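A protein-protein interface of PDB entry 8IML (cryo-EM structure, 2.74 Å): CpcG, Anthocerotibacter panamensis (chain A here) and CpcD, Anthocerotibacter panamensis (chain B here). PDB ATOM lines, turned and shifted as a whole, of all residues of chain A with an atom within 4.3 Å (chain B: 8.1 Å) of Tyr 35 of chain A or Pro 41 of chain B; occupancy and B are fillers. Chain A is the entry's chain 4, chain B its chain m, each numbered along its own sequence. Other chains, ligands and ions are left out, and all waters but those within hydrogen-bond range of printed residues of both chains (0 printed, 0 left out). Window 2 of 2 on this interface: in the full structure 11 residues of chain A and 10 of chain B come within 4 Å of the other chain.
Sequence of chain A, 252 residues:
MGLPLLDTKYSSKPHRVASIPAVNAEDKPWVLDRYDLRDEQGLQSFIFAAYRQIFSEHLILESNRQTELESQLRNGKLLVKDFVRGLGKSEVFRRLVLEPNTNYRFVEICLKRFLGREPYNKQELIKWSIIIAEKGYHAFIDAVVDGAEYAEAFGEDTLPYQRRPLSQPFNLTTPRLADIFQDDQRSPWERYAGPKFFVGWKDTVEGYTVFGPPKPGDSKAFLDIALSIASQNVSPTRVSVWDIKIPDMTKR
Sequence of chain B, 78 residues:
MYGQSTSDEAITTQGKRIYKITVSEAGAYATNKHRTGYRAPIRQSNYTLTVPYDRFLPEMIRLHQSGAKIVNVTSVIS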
ATOM      1  N   VAL A  31     -31.245  17.095  13.323  1.00  0.00           N
ATOM      2  CA  VAL A  31     -31.478  16.515  14.637  1.00  0.00           C
ATOM      3  C   VAL A  31     -30.932  17.514  15.651  1.00  0.00           C
ATOM      4  O   VAL A  31     -29.758  17.479  16.024  1.00  0.00           O
ATOM      5  CB  VAL A  31     -30.829  15.141  14.765  1.00  0.00           C
ATOM      6  CG1 VAL A  31     -31.205  14.496  16.070  1.00  0.00           C
ATOM      7  CG2 VAL A  31     -31.242  14.263  13.597  1.00  0.00           C
ATOM      8  N   ASP A  33     -30.554  19.177  19.380  1.00  0.00           N
ATOM      9  CA  ASP A  33     -30.297  18.459  20.617  1.00  0.00           C
ATOM     10  C   ASP A  33     -29.891  19.450  21.699  1.00  0.00           C
ATOM     11  O   ASP A  33     -30.031  20.665  21.544  1.00  0.00           O
ATOM     12  CB  ASP A  33     -29.229  17.387  20.384  1.00  0.00           C
ATOM     13  CG  ASP A  33     -29.294  16.263  21.396  1.00  0.00           C
ATOM     14  OD1 ASP A  33     -30.115  16.353  22.328  1.00  0.00           O
ATOM     15  OD2 ASP A  33     -28.526  15.290  21.258  1.00  0.00           O
ATOM     16  N   ARG A  34     -29.387  18.910  22.812  1.00  0.00           N
ATOM     17  CA  ARG A  34     -28.977  19.740  23.939  1.00  0.00           C
ATOM     18  C   ARG A  34     -27.766  20.599  23.594  1.00  0.00           C
ATOM     19  O   ARG A  34     -27.685  21.759  24.011  1.00  0.00           O
ATOM     20  CB  ARG A  34     -28.676  18.861  25.151  1.00  0.00           C
ATOM     21  CG  ARG A  34     -28.597  19.615  26.466  1.00  0.00           C
ATOM     22  CD  ARG A  34     -29.820  20.493  26.664  1.00  0.00           C
ATOM     23  NE  ARG A  34     -30.187  20.622  28.070  1.00  0.00           N
ATOM     24  CZ  ARG A  34     -31.401  20.953  28.496  1.00  0.00           C
ATOM     25  NH1 ARG A  34     -31.647  21.046  29.795  1.00  0.00           N
ATOM     26  NH2 ARG A  34     -32.369  21.191  27.623  1.00  0.00           N
ATOM     27  N   TYR A  35     -26.809  20.042  22.846  1.00  0.00           N
ATOM     28  CA  TYR A  35     -25.591  20.789  22.547  1.00  0.00           C
ATOM     29  C   TYR A  35     -25.886  22.058  21.760  1.00  0.00           C
ATOM     30  O   TYR A  35     -25.256  23.097  22.001  1.00  0.00           O
ATOM     31  CB  TYR A  35     -24.592  19.901  21.800  1.00  0.00           C
ATOM     32  CG  TYR A  35     -25.106  19.287  20.516  1.00  0.00           C
ATOM     33  CD1 TYR A  35     -25.161  20.024  19.338  1.00  0.00           C
ATOM     34  CD2 TYR A  35     -25.513  17.961  20.476  1.00  0.00           C
ATOM     35  CE1 TYR A  35     -25.630  19.463  18.167  1.00  0.00           C
ATOM     36  CE2 TYR A  35     -25.973  17.390  19.307  1.00  0.00           C
ATOM     37  CZ  TYR A  35     -26.033  18.145  18.156  1.00  0.00           C
ATOM     38  OH  TYR A  35     -26.495  17.580  16.991  1.00  0.00           O
ATOM     39  N   ASP A  36     -26.856  22.008  20.846  1.00  0.00           N
ATOM     40  CA  ASP A  36     -27.239  23.189  20.083  1.00  0.00           C
ATOM     41  C   ASP A  36     -27.703  24.321  20.987  1.00  0.00           C
ATOM     42  O   ASP A  36     -27.669  25.486  20.578  1.00  0.00           O
ATOM     43  CB  ASP A  36     -28.341  22.820  19.086  1.00  0.00           C
ATOM     44  CG  ASP A  36     -28.331  23.694  17.849  1.00  0.00           C
ATOM     45  OD1 ASP A  36     -28.311  24.934  17.986  1.00  0.00           O
ATOM     46  OD2 ASP A  36     -28.345  23.138  16.732  1.00  0.00           O
ATOM     47  N   LEU A  37     -28.115  24.003  22.212  1.00  0.00           N
ATOM     48  CA  LEU A  37     -28.605  25.013  23.139  1.00  0.00           C
ATOM     49  C   LEU A  37     -27.472  25.769  23.821  1.00  0.00           C
ATOM     50  O   LEU A  37     -27.716  26.801  24.455  1.00  0.00           O
ATOM     51  CB  LEU A  37     -29.497  24.358  24.193  1.00  0.00           C
ATOM     52  CG  LEU A  37     -30.981  24.147  23.895  1.00  0.00           C
ATOM     53  CD1 LEU A  37     -31.179  23.428  22.589  1.00  0.00           C
ATOM     54  CD2 LEU A  37     -31.604  23.344  25.019  1.00  0.00           C
ATOM     55  N   ARG A  38     -26.235  25.279  23.706  1.00  0.00           N
ATOM     56  CA  ARG A  38     -25.136  25.902  24.437  1.00  0.00           C
ATOM     57  C   ARG A  38     -24.761  27.254  23.842  1.00  0.00           C
ATOM     58  O   ARG A  38     -24.481  28.206  24.579  1.00  0.00           O
ATOM     59  CB  ARG A  38     -23.938  24.956  24.483  1.00  0.00           C
ATOM     60  CG  ARG A  38     -24.157  23.816  25.462  1.00  0.00           C
ATOM     61  CD  ARG A  38     -22.971  22.883  25.568  1.00  0.00           C
ATOM     62  NE  ARG A  38     -23.114  21.989  26.716  1.00  0.00           N
ATOM     63  CZ  ARG A  38     -23.821  20.864  26.709  1.00  0.00           C
ATOM     64  NH1 ARG A  38     -23.894  20.120  27.805  1.00  0.00           N
ATOM     65  NH2 ARG A  38     -24.459  20.484  25.613  1.00  0.00           N
ATOM     66  N   GLU B  25     -24.853   9.025  35.571  1.00  0.00           N
ATOM     67  CA  GLU B  25     -25.119   7.885  34.693  1.00  0.00           C
ATOM     68  C   GLU B  25     -24.030   6.823  34.784  1.00  0.00           C
ATOM     69  O   GLU B  25     -23.656   6.194  33.789  1.00  0.00           O
ATOM     70  CB  GLU B  25     -25.324   8.358  33.256  1.00  0.00           C
ATOM     71  CG  GLU B  25     -24.098   8.853  32.515  1.00  0.00           C
ATOM     72  CD  GLU B  25     -24.461   9.750  31.350  1.00  0.00           C
ATOM     73  OE1 GLU B  25     -25.467   9.457  30.670  1.00  0.00           O
ATOM     74  OE2 GLU B  25     -23.743  10.737  31.103  1.00  0.00           O
ATOM     75  N   TYR B  38     -26.478   3.542  21.522  1.00  0.00           N
ATOM     76  CA  TYR B  38     -26.605   4.991  21.641  1.00  0.00           C
ATOM     77  C   TYR B  38     -27.295   5.535  20.396  1.00  0.00           C
ATOM     78  O   TYR B  38     -26.829   5.320  19.273  1.00  0.00           O
ATOM     79  CB  TYR B  38     -25.239   5.644  21.831  1.00  0.00           C
ATOM     80  CG  TYR B  38     -24.614   5.387  23.183  1.00  0.00           C
ATOM     81  CD1 TYR B  38     -25.071   6.049  24.315  1.00  0.00           C
ATOM     82  CD2 TYR B  38     -23.562   4.493  23.326  1.00  0.00           C
ATOM     83  CE1 TYR B  38     -24.503   5.821  25.552  1.00  0.00           C
ATOM     84  CE2 TYR B  38     -22.986   4.259  24.559  1.00  0.00           C
ATOM     85  CZ  TYR B  38     -23.461   4.928  25.669  1.00  0.00           C
ATOM     86  OH  TYR B  38     -22.892   4.700  26.900  1.00  0.00           O
ATOM     87  N   ARG B  39     -28.412   6.237  20.597  1.00  0.00           N
ATOM     88  CA  ARG B  39     -29.068   6.923  19.490  1.00  0.00           C
ATOM     89  C   ARG B  39     -28.628   8.377  19.392  1.00  0.00           C
ATOM     90  O   ARG B  39     -28.765   8.993  18.328  1.00  0.00           O
ATOM     91  CB  ARG B  39     -30.589   6.846  19.645  1.00  0.00           C
ATOM     92  CG  ARG B  39     -31.102   5.518  20.176  1.00  0.00           C
ATOM     93  CD  ARG B  39     -32.603   5.574  20.414  1.00  0.00           C
ATOM     94  NE  ARG B  39     -33.076   4.491  21.273  1.00  0.00           N
ATOM     95  CZ  ARG B  39     -33.477   3.304  20.832  1.00  0.00           C
ATOM     96  NH1 ARG B  39     -33.465   3.037  19.533  1.00  0.00           N
ATOM     97  NH2 ARG B  39     -33.892   2.382  21.692  1.00  0.00           N
ATOM     98  N   ALA B  40     -28.100   8.930  20.474  1.00  0.00           N
ATOM     99  CA  ALA B  40     -27.735  10.331  20.592  1.00  0.00           C
ATOM    100  C   ALA B  40     -26.313  10.447  21.114  1.00  0.00           C
ATOM    101  O   ALA B  40     -25.788   9.507  21.720  1.00  0.00           O
ATOM    102  CB  ALA B  40     -28.701  11.070  21.531  1.00  0.00           C
ATOM    103  N   PRO B  41     -25.652  11.585  20.881  1.00  0.00           N
ATOM    104  CA  PRO B  41     -24.308  11.778  21.439  1.00  0.00           C
ATOM    105  C   PRO B  41     -24.320  11.727  22.960  1.00  0.00           C
ATOM    106  O   PRO B  41     -25.293  12.115  23.612  1.00  0.00           O
ATOM    107  CB  PRO B  41     -23.903  13.167  20.926  1.00  0.00           C
ATOM    108  CG  PRO B  41     -25.185  13.823  20.512  1.00  0.00           C
ATOM    109  CD  PRO B  41     -26.053  12.710  20.020  1.00  0.00           C
ATOM    110  N   ILE B  42     -23.220  11.240  23.519  1.00  0.00           N
ATOM    111  CA  ILE B  42     -23.131  10.971  24.949  1.00  0.00           C
ATOM    112  C   ILE B  42     -22.778  12.249  25.700  1.00  0.00           C
ATOM    113  O   ILE B  42     -21.878  12.999  25.302  1.00  0.00           O
ATOM    114  CB  ILE B  42     -22.107   9.856  25.215  1.00  0.00           C
ATOM    115  CG1 ILE B  42     -22.527   8.586  24.473  1.00  0.00           C
ATOM    116  CG2 ILE B  42     -21.976   9.591  26.708  1.00  0.00           C
ATOM    117  CD1 ILE B  42     -21.444   7.550  24.359  1.00  0.00           C
ATOM    118  N   ARG B  43     -23.491  12.494  26.793  1.00  0.00           N
ATOM    119  CA  ARG B  43     -23.338  13.686  27.614  1.00  0.00           C
ATOM    120  C   ARG B  43     -22.637  13.340  28.922  1.00  0.00           C
ATOM    121  O   ARG B  43     -22.333  12.180  29.208  1.00  0.00           O
ATOM    122  CB  ARG B  43     -24.705  14.324  27.889  1.00  0.00           C
ATOM    123  CG  ARG B  43     -25.181  15.278  26.800  1.00  0.00           C
ATOM    124  CD  ARG B  43     -24.556  16.661  26.939  1.00  0.00           C
ATOM    125  NE  ARG B  43     -24.393  17.077  28.332  1.00  0.00           N
ATOM    126  CZ  ARG B  43     -25.393  17.359  29.164  1.00  0.00           C
ATOM    127  NH1 ARG B  43     -26.652  17.286  28.753  1.00  0.00           N
ATOM    128  NH2 ARG B  43     -25.132  17.725  30.411  1.00  0.00           N
ATOM    129  N   GLN B  44     -22.377  14.373  29.720  1.00  0.00           N
ATOM    130  CA  GLN B  44     -21.701  14.188  30.996  1.00  0.00           C
ATOM    131  C   GLN B  44     -22.586  13.425  31.976  1.00  0.00           C
ATOM    132  O   GLN B  44     -23.817  13.444  31.884  1.00  0.00           O
ATOM    133  CB  GLN B  44     -21.298  15.537  31.593  1.00  0.00           C
ATOM    134  CG  GLN B  44     -20.671  16.495  30.595  1.00  0.00           C
ATOM    135  CD  GLN B  44     -21.693  17.382  29.923  1.00  0.00           C
ATOM    136  OE1 GLN B  44     -22.686  17.776  30.534  1.00  0.00           O
ATOM    137  NE2 GLN B  44     -21.460  17.698  28.654  1.00  0.00           N
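Of the 8 printed residues of chain B, 3 touch a printed residue of chain A.
Hydrophobic or aromatic side chains of chain B that line the printed part of chain A: Pro 41.
Of the 7 printed residues of chain A, 4 touch a printed residue of chain B.
Hydrophobic or aromatic side chains of chain A within 4 Å of the printed part of chain B: Tyr 35.
Among the printed residues, 5 pairs touch across the chains.
Among the printed residues, no Asp or Glu carboxylate lies within 4 Å of a Lys or Arg side-chain nitrogen of the other chain.
Among the printed residues, merely in contact across the chains: Arg 38 of chain A with Gln 44 of chain B (3.5 Å), Asp 33 of chain A with Pro 41 of chain B (3.7 Å), Arg 34 of chain A with Arg 43 of chain B (3.8 Å) and Tyr 35 of chain A with Pro 41 of chain B (3.8 Å).
Of the printed residues of chain B, Asp 33 of chain A touches Pro 41.
Printed residues of chain B within 4 Å of Arg 34 of chain A: Arg 43.
Of chain B, only Pro 41 (3.8 Å) comes within 4 Å of Tyr 35 of chain A.
Of the printed residues of chain B, Arg 38 of chain A touches Arg 43 and Gln 44.
Of chain A, only Asp 33 and Tyr 35 come within 4 Å of Pro 41 of chain B.
The nearest printed residue of chain A that does not touch Pro 41 of chain B is Val 31 of chain A (6.7 Å).
NH2 of Arg 43 of chain B lies within hydrogen-bond range of OE1 of Gln 44 of chain B (2.4 Å).
OH of Tyr 35 of chain A is in hydrogen-bond range of O of Val 31 of chain A, at 3.4 Å.
The guanidinium group (NE) of Arg 43 of chain B lies close to the guanidinium group (NH1) of Arg 38 of chain A.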
